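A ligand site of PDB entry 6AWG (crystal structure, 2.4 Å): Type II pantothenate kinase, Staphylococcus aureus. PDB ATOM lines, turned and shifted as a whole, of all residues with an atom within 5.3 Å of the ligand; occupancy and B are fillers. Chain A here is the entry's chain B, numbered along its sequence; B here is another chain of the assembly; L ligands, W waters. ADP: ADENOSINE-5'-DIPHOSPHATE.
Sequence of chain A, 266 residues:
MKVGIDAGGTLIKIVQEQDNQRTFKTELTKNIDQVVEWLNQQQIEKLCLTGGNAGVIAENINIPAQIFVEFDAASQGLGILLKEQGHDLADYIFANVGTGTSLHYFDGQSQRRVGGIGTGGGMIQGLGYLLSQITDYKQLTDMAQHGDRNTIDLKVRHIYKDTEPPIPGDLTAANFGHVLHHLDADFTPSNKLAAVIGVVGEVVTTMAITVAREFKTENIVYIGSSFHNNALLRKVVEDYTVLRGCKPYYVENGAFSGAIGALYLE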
ATOM      1  N   ASP A   6      25.746 -19.479 -16.358  1.00  0.00           N
ATOM      2  CA  ASP A   6      24.355 -19.123 -16.725  1.00  0.00           C
ATOM      3  C   ASP A   6      23.514 -20.156 -16.000  1.00  0.00           C
ATOM      4  O   ASP A   6      23.477 -21.333 -16.394  1.00  0.00           O
ATOM      5  CB  ASP A   6      24.110 -19.153 -18.241  1.00  0.00           C
ATOM      6  CG  ASP A   6      22.621 -18.862 -18.668  1.00  0.00           C
ATOM      7  OD1 ASP A   6      21.712 -18.730 -17.813  1.00  0.00           O
ATOM      8  OD2 ASP A   6      22.347 -18.763 -19.899  1.00  0.00           O
ATOM      9  N   ALA A   7      22.844 -19.722 -14.932  1.00  0.00           N
ATOM     10  CA  ALA A   7      22.113 -20.631 -14.079  1.00  0.00           C
ATOM     11  C   ALA A   7      20.653 -20.554 -14.470  1.00  0.00           C
ATOM     12  O   ALA A   7      19.933 -19.649 -14.013  1.00  0.00           O
ATOM     13  CB  ALA A   7      22.310 -20.281 -12.592  1.00  0.00           C
ATOM     14  N   GLY A   8      20.223 -21.506 -15.294  1.00  0.00           N
ATOM     15  CA  GLY A   8      18.828 -21.560 -15.769  1.00  0.00           C
ATOM     16  C   GLY A   8      17.738 -22.237 -14.925  1.00  0.00           C
ATOM     17  O   GLY A   8      17.907 -22.720 -13.778  1.00  0.00           O
ATOM     18  N   GLY A   9      16.562 -22.272 -15.521  1.00  0.00           N
ATOM     19  CA  GLY A   9      15.442 -22.970 -14.946  1.00  0.00           C
ATOM     20  C   GLY A   9      15.741 -24.460 -14.764  1.00  0.00           C
ATOM     21  O   GLY A   9      15.339 -25.047 -13.761  1.00  0.00           O
ATOM     22  N   THR A  10      16.463 -25.073 -15.710  1.00  0.00           N
ATOM     23  CA  THR A  10      16.734 -26.511 -15.652  1.00  0.00           C
ATOM     24  C   THR A  10      18.219 -26.862 -15.592  1.00  0.00           C
ATOM     25  O   THR A  10      18.579 -27.811 -14.893  1.00  0.00           O
ATOM     26  CB  THR A  10      16.113 -27.260 -16.829  1.00  0.00           C
ATOM     27  OG1 THR A  10      14.794 -26.764 -17.097  1.00  0.00           O
ATOM     28  CG2 THR A  10      16.045 -28.778 -16.537  1.00  0.00           C
ATOM     29  N   LEU A  11      19.060 -26.156 -16.321  1.00  0.00           N
ATOM     30  CA  LEU A  11      20.482 -26.448 -16.337  1.00  0.00           C
ATOM     31  C   LEU A  11      21.374 -25.217 -15.962  1.00  0.00           C
ATOM     32  O   LEU A  11      21.051 -24.044 -16.276  1.00  0.00           O
ATOM     33  CB  LEU A  11      20.924 -26.986 -17.696  1.00  0.00           C
ATOM     34  CG  LEU A  11      20.177 -28.204 -18.260  1.00  0.00           C
ATOM     35  CD1 LEU A  11      20.428 -28.465 -19.758  1.00  0.00           C
ATOM     36  CD2 LEU A  11      20.540 -29.446 -17.456  1.00  0.00           C
ATOM     37  N   LYS A  13      25.036 -23.768 -16.776  1.00  0.00           N
ATOM     38  CA  LYS A  13      26.066 -23.848 -17.791  1.00  0.00           C
ATOM     39  C   LYS A  13      27.278 -23.072 -17.254  1.00  0.00           C
ATOM     40  O   LYS A  13      27.172 -21.908 -16.913  1.00  0.00           O
ATOM     41  CB  LYS A  13      25.539 -23.288 -19.129  1.00  0.00           C
ATOM     42  CG  LYS A  13      24.462 -24.135 -19.872  1.00  0.00           C
ATOM     43  CD  LYS A  13      23.046 -24.211 -19.243  1.00  0.00           C
ATOM     44  CE  LYS A  13      22.322 -22.900 -19.336  1.00  0.00           C
ATOM     45  NZ  LYS A  13      20.933 -23.025 -18.853  1.00  0.00           N
ATOM     46  N   LEU A  28      22.836 -29.970 -13.333  1.00  0.00           N
ATOM     47  CA  LEU A  28      21.403 -29.750 -13.161  1.00  0.00           C
ATOM     48  C   LEU A  28      21.193 -28.603 -12.144  1.00  0.00           C
ATOM     49  O   LEU A  28      21.925 -28.455 -11.161  1.00  0.00           O
ATOM     50  CB  LEU A  28      20.692 -31.038 -12.750  1.00  0.00           C
ATOM     51  CG  LEU A  28      20.740 -32.266 -13.706  1.00  0.00           C
ATOM     52  CD1 LEU A  28      20.310 -33.584 -13.068  1.00  0.00           C
ATOM     53  CD2 LEU A  28      19.889 -32.043 -14.940  1.00  0.00           C
ATOM     54  N   THR A  29      20.180 -27.780 -12.414  1.00  0.00           N
ATOM     55  CA  THR A  29      19.753 -26.754 -11.492  1.00  0.00           C
ATOM     56  C   THR A  29      19.403 -27.397 -10.142  1.00  0.00           C
ATOM     57  O   THR A  29      19.821 -26.921  -9.091  1.00  0.00           O
ATOM     58  CB  THR A  29      18.592 -25.968 -12.101  1.00  0.00           C
ATOM     59  OG1 THR A  29      19.077 -25.276 -13.261  1.00  0.00           O
ATOM     60  CG2 THR A  29      17.989 -24.953 -11.108  1.00  0.00           C
ATOM     61  N   ASN A  96      16.367 -18.364 -28.329  1.00  0.00           N
ATOM     62  CA  ASN A  96      16.915 -19.047 -27.194  1.00  0.00           C
ATOM     63  C   ASN A  96      15.952 -20.056 -26.591  1.00  0.00           C
ATOM     64  O   ASN A  96      15.077 -19.699 -25.777  1.00  0.00           O
ATOM     65  CB  ASN A  96      17.316 -18.001 -26.165  1.00  0.00           C
ATOM     66  CG  ASN A  96      18.265 -18.575 -25.143  1.00  0.00           C
ATOM     67  OD1 ASN A  96      18.347 -19.807 -24.988  1.00  0.00           O
ATOM     68  ND2 ASN A  96      18.987 -17.698 -24.447  1.00  0.00           N
ATOM     69  N   VAL A  97      16.119 -21.323 -26.943  1.00  0.00           N
ATOM     70  CA  VAL A  97      15.116 -22.366 -26.635  1.00  0.00           C
ATOM     71  C   VAL A  97      15.513 -23.126 -25.390  1.00  0.00           C
ATOM     72  O   VAL A  97      16.139 -24.187 -25.455  1.00  0.00           O
ATOM     73  CB  VAL A  97      14.929 -23.309 -27.849  1.00  0.00           C
ATOM     74  CG1 VAL A  97      13.828 -24.316 -27.626  1.00  0.00           C
ATOM     75  CG2 VAL A  97      14.592 -22.495 -29.095  1.00  0.00           C
ATOM     76  N   GLY A  98      15.125 -22.601 -24.234  1.00  0.00           N
ATOM     77  CA  GLY A  98      15.528 -23.195 -22.936  1.00  0.00           C
ATOM     78  C   GLY A  98      14.442 -24.020 -22.266  1.00  0.00           C
ATOM     79  O   GLY A  98      13.786 -24.862 -22.904  1.00  0.00           O
ATOM     80  N   THR A  99      14.213 -23.745 -20.988  1.00  0.00           N
ATOM     81  CA  THR A  99      13.092 -24.333 -20.289  1.00  0.00           C
ATOM     82  C   THR A  99      11.835 -23.812 -20.955  1.00  0.00           C
ATOM     83  O   THR A  99      10.872 -24.577 -21.178  1.00  0.00           O
ATOM     84  CB  THR A  99      13.089 -23.968 -18.804  1.00  0.00           C
ATOM     85  OG1 THR A  99      14.360 -24.301 -18.233  1.00  0.00           O
ATOM     86  CG2 THR A  99      12.064 -24.771 -18.091  1.00  0.00           C
ATOM     87  N   GLY A 100      11.877 -22.510 -21.233  1.00  0.00           N
ATOM     88  CA  GLY A 100      10.958 -21.791 -22.104  1.00  0.00           C
ATOM     89  C   GLY A 100      11.713 -21.077 -23.221  1.00  0.00           C
ATOM     90  O   GLY A 100      12.935 -20.967 -23.193  1.00  0.00           O
ATOM     91  N   GLY A 121      11.968 -26.563 -24.061  1.00  0.00           N
ATOM     92  CA  GLY A 121      12.517 -27.736 -23.414  1.00  0.00           C
ATOM     93  C   GLY A 121      11.726 -28.204 -22.219  1.00  0.00           C
ATOM     94  O   GLY A 121      11.543 -29.414 -22.036  1.00  0.00           O
ATOM     95  N   GLY A 122      11.256 -27.262 -21.415  1.00  0.00           N
ATOM     96  CA  GLY A 122      10.440 -27.580 -20.240  1.00  0.00           C
ATOM     97  C   GLY A 122       9.148 -28.340 -20.608  1.00  0.00           C
ATOM     98  O   GLY A 122       8.744 -29.218 -19.854  1.00  0.00           O
ATOM     99  N   ILE A 124       8.539 -30.221 -23.512  1.00  0.00           N
ATOM    100  CA  ILE A 124       9.027 -31.562 -23.905  1.00  0.00           C
ATOM    101  C   ILE A 124       9.119 -32.508 -22.649  1.00  0.00           C
ATOM    102  O   ILE A 124       8.523 -33.606 -22.599  1.00  0.00           O
ATOM    103  CB  ILE A 124      10.387 -31.423 -24.646  1.00  0.00           C
ATOM    104  CG1 ILE A 124      10.197 -30.779 -26.022  1.00  0.00           C
ATOM    105  CG2 ILE A 124      11.044 -32.784 -24.836  1.00  0.00           C
ATOM    106  CD1 ILE A 124      11.434 -30.178 -26.704  1.00  0.00           C
ATOM    107  N   GLN A 125       9.840 -32.043 -21.635  1.00  0.00           N
ATOM    108  CA  GLN A 125      10.040 -32.822 -20.418  1.00  0.00           C
ATOM    109  C   GLN A 125       8.760 -33.136 -19.639  1.00  0.00           C
ATOM    110  O   GLN A 125       8.578 -34.247 -19.209  1.00  0.00           O
ATOM    111  CB  GLN A 125      11.000 -32.091 -19.497  1.00  0.00           C
ATOM    112  CG  GLN A 125      12.426 -32.259 -19.943  1.00  0.00           C
ATOM    113  CD  GLN A 125      13.386 -31.759 -18.903  1.00  0.00           C
ATOM    114  OE1 GLN A 125      13.502 -30.565 -18.723  1.00  0.00           O
ATOM    115  NE2 GLN A 125      14.076 -32.653 -18.242  1.00  0.00           N
ATOM    116  N   TYR A 137      15.875 -37.686 -19.063  1.00  0.00           N
ATOM    117  CA  TYR A 137      15.858 -36.841 -20.250  1.00  0.00           C
ATOM    118  C   TYR A 137      16.455 -37.514 -21.493  1.00  0.00           C
ATOM    119  O   TYR A 137      15.942 -37.330 -22.595  1.00  0.00           O
ATOM    120  CB  TYR A 137      16.586 -35.520 -19.975  1.00  0.00           C
ATOM    121  CG  TYR A 137      16.763 -34.706 -21.228  1.00  0.00           C
ATOM    122  CD1 TYR A 137      15.740 -33.948 -21.731  1.00  0.00           C
ATOM    123  CD2 TYR A 137      17.943 -34.738 -21.944  1.00  0.00           C
ATOM    124  CE1 TYR A 137      15.899 -33.207 -22.894  1.00  0.00           C
ATOM    125  CE2 TYR A 137      18.086 -33.992 -23.092  1.00  0.00           C
ATOM    126  CZ  TYR A 137      17.071 -33.224 -23.551  1.00  0.00           C
ATOM    127  OH  TYR A 137      17.249 -32.464 -24.668  1.00  0.00           O
ATOM    128  N   GLY A 224      20.084 -22.949 -27.187  1.00  0.00           N
ATOM    129  CA  GLY A 224      19.445 -23.517 -26.021  1.00  0.00           C
ATOM    130  C   GLY A 224      19.802 -24.996 -25.927  1.00  0.00           C
ATOM    131  O   GLY A 224      20.201 -25.632 -26.938  1.00  0.00           O
ATOM    132  N   SER A 225      19.684 -25.538 -24.723  1.00  0.00           N
ATOM    133  CA  SER A 225      19.987 -26.966 -24.516  1.00  0.00           C
ATOM    134  C   SER A 225      18.845 -27.874 -24.953  1.00  0.00           C
ATOM    135  O   SER A 225      19.022 -29.068 -24.994  1.00  0.00           O
ATOM    136  CB  SER A 225      20.310 -27.232 -23.045  1.00  0.00           C
ATOM    137  OG  SER A 225      21.388 -26.392 -22.622  1.00  0.00           O
ATOM    138  N   SER A 226      17.675 -27.322 -25.269  1.00  0.00           N
ATOM    139  CA  SER A 226      16.562 -28.090 -25.804  1.00  0.00           C
ATOM    140  C   SER A 226      16.883 -28.940 -27.041  1.00  0.00           C
ATOM    141  O   SER A 226      16.182 -29.886 -27.338  1.00  0.00           O
ATOM    142  CB  SER A 226      15.381 -27.163 -26.102  1.00  0.00           C
ATOM    143  OG  SER A 226      14.941 -26.501 -24.930  1.00  0.00           O
ATOM    144  N   HIS A 228      19.822 -30.626 -27.329  1.00  0.00           N
ATOM    145  CA  HIS A 228      20.769 -31.695 -26.973  1.00  0.00           C
ATOM    146  C   HIS A 228      20.102 -33.023 -26.966  1.00  0.00           C
ATOM    147  O   HIS A 228      19.014 -33.197 -26.413  1.00  0.00           O
ATOM    148  CB  HIS A 228      21.422 -31.453 -25.599  1.00  0.00           C
ATOM    149  CG  HIS A 228      22.378 -30.292 -25.592  1.00  0.00           C
ATOM    150  ND1 HIS A 228      23.006 -29.833 -26.736  1.00  0.00           N
ATOM    151  CD2 HIS A 228      22.822 -29.512 -24.581  1.00  0.00           C
ATOM    152  CE1 HIS A 228      23.780 -28.804 -26.428  1.00  0.00           C
ATOM    153  NE2 HIS A 228      23.687 -28.585 -25.129  1.00  0.00           N
ATOM    154  N   ALA A 255      24.210 -23.261 -26.331  1.00  0.00           N
ATOM    155  CA  ALA A 255      23.692 -23.349 -24.951  1.00  0.00           C
ATOM    156  C   ALA A 255      24.510 -22.585 -23.870  1.00  0.00           C
ATOM    157  O   ALA A 255      23.952 -22.257 -22.797  1.00  0.00           O
ATOM    158  CB  ALA A 255      23.645 -24.797 -24.547  1.00  0.00           C
ATOM    159  N   ILE B 159      11.551 -19.382 -11.916  1.00  0.00           N
ATOM    160  CA  ILE B 159      12.843 -19.441 -12.489  1.00  0.00           C
ATOM    161  C   ILE B 159      13.760 -18.393 -11.880  1.00  0.00           C
ATOM    162  O   ILE B 159      14.838 -18.707 -11.516  1.00  0.00           O
ATOM    163  CB  ILE B 159      12.790 -19.272 -14.018  1.00  0.00           C
ATOM    164  CG1 ILE B 159      12.038 -20.432 -14.678  1.00  0.00           C
ATOM    165  CG2 ILE B 159      14.167 -19.084 -14.585  1.00  0.00           C
ATOM    166  CD1 ILE B 159      12.095 -20.450 -16.181  1.00  0.00           C
HETATM  167  PB  ADP L   1      17.513 -23.027 -18.920  1.00  0.00           P
HETATM  168  O1B ADP L   1      18.492 -21.862 -19.008  1.00  0.00           O
HETATM  169  O2B ADP L   1      18.043 -24.123 -18.027  1.00  0.00           O
HETATM  170  O3B ADP L   1      16.125 -22.586 -18.545  1.00  0.00           O
HETATM  171  PA  ADP L   1      18.513 -24.472 -21.246  1.00  0.00           P
HETATM  172  O1A ADP L   1      19.042 -23.697 -22.412  1.00  0.00           O
HETATM  173  O2A ADP L   1      19.580 -25.129 -20.399  1.00  0.00           O
HETATM  174  O3A ADP L   1      17.399 -23.611 -20.426  1.00  0.00           O
HETATM  175  O5' ADP L   1      17.540 -25.675 -21.746  1.00  0.00           O
HETATM  176  C5' ADP L   1      17.026 -26.596 -20.758  1.00  0.00           C
HETATM  177  C4' ADP L   1      16.235 -27.695 -21.489  1.00  0.00           C
HETATM  178  O4' ADP L   1      17.116 -28.468 -22.268  1.00  0.00           O
HETATM  179  C3' ADP L   1      15.443 -28.679 -20.644  1.00  0.00           C
HETATM  180  O3' ADP L   1      14.111 -28.211 -20.456  1.00  0.00           O
HETATM  181  C2' ADP L   1      15.472 -29.931 -21.499  1.00  0.00           C
HETATM  182  O2' ADP L   1      14.446 -29.921 -22.487  1.00  0.00           O
HETATM  183  C1' ADP L   1      16.748 -29.839 -22.267  1.00  0.00           C
HETATM  184  N9  ADP L   1      17.842 -30.641 -21.690  1.00  0.00           N
HETATM  185  C8  ADP L   1      18.990 -30.835 -22.369  1.00  0.00           C
HETATM  186  N7  ADP L   1      19.834 -31.602 -21.654  1.00  0.00           N
HETATM  187  C5  ADP L   1      19.214 -31.905 -20.504  1.00  0.00           C
HETATM  188  C6  ADP L   1      19.549 -32.638 -19.292  1.00  0.00           C
HETATM  189  N6  ADP L   1      20.735 -33.250 -19.251  1.00  0.00           N
HETATM  190  N1  ADP L   1      18.698 -32.703 -18.257  1.00  0.00           N
HETATM  191  C2  ADP L   1      17.507 -32.100 -18.288  1.00  0.00           C
HETATM  192  N3  ADP L   1      17.140 -31.380 -19.378  1.00  0.00           N
HETATM  193  C4  ADP L   1      17.922 -31.254 -20.502  1.00  0.00           C
HETATM  194  O   HOH W   1      22.665 -30.977 -22.014  1.00  0.00           O
HETATM  195  O   HOH W   2      15.891 -20.024 -18.173  1.00  0.00           O
HETATM  196  O   HOH W   3      18.055 -20.969 -22.404  1.00  0.00           O
HETATM  197  O   HOH W   4      19.378 -18.746 -18.482  1.00  0.00           O
HETATM  198  O   HOH W   5      14.205 -20.445 -20.496  1.00  0.00           O
HETATM  199  O   HOH W   6      20.555 -20.506 -20.416  1.00  0.00           O
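An oxygen (O2A) of the ligand lies within hydrogen-bond range of the side-chain hydroxyl (OG) of Ser 225, at 3.1 Å. O3B of the ligand is in hydrogen-bond range of N of Gly 9 (3.1 Å). An oxygen (O2') of the ligand is in hydrogen-bond range of the backbone carbonyl oxygen (O) of Gly 121, at 3.0 Å. O3' of the ligand sits at hydrogen-bond distance from OE1 of Gln 125. An oxygen (O3A) of the ligand sits at hydrogen-bond distance from the backbone NH (N) of Thr 99 (3.2 Å). An oxygen (O2B) of the ligand sits at hydrogen-bond distance from the backbone NH of Leu 11 (2.8 Å). N of Gly 122 sits at hydrogen-bond distance from O3' of the ligand. O1B of the ligand lies within salt-bridge range of NZ of Lys 13 (2.7 Å). An oxygen (O4') of the ligand lies within hydrogen-bond range of the backbone NH (N) of Ser 226. O1A of the ligand sits at hydrogen-bond distance from N of Ser 225, 3.0 Å away. An oxygen (O2B) of the ligand is in hydrogen-bond range of the backbone NH (N) of Thr 10 (3.0 Å). An oxygen (O3B) of the ligand lies within hydrogen-bond range of the side-chain hydroxyl (OG1) of Thr 99.
Water W6 lies within hydrogen-bond range of the side-chain carboxylate of Asp 6, an oxygen (O1B) of the ligand and the side-chain amino group of Lys 13. Water W3 lies within hydrogen-bond range of OD1 of Asn 96 (2.8 Å) and O1A of the ligand (2.9 Å). Water W4 lies within hydrogen-bond range of the side-chain carboxylate (OD1) of Asp 6 (2.4 Å) and an oxygen (O1B) of the ligand (3.3 Å). Water W5 lies within hydrogen-bond range of the backbone carbonyl oxygen of Gly 100, the backbone NH of Thr 99 and an oxygen (O3B) of the ligand.
Gly 8 touches the ligand (CA to O1B, 3.3 Å). Leu 28 touches the ligand (CD2 to N1, 3.6 Å). Gly 98 touches the ligand (CA to O3A, 3.2 Å). CZ of Tyr 137 touches N9 of the ligand (3.3 Å). Gly 224 touches the ligand. Hydrophobic or aromatic side chains that line the ligand: Leu 11, Leu 28 and Tyr 137. 15 residues have an atom within 4 Å of the ligand: Gly 8, Gly 9, Thr 10, Leu 11, Lys 13, Leu 28, Gly 98, Thr 99, Gly 121, Gly 122, Gln 125, Tyr 137, Gly 224, Ser 225 and Ser 226.
The side-chain hydroxyl (OG) of Ser 226 sits at hydrogen-bond distance from the backbone carbonyl oxygen (O) of Gly 98, at 2.9 Å. O of Thr 10 sits at hydrogen-bond distance from N of Thr 29 (3.0 Å). NZ of Lys 13 sits at hydrogen-bond distance from O of Leu 11 (2.8 Å). The backbone NH (N) of Gly 121 is in hydrogen-bond range of the backbone carbonyl oxygen (O) of Gly 98. The side-chain hydroxyl (OG) of Ser 226 sits at hydrogen-bond distance from the backbone NH (N) of Gly 121, at 3.1 Å. The backbone NH of Leu 11 sits at hydrogen-bond distance from the side-chain hydroxyl of Thr 29 (3.2 Å). The backbone carbonyl oxygen of Val 97 sits at hydrogen-bond distance from the side-chain hydroxyl of Ser 226, at 2.7 Å. The backbone carbonyl oxygen (O) of Gly 8 sits at hydrogen-bond distance from the side-chain hydroxyl (OG1) of Thr 29.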
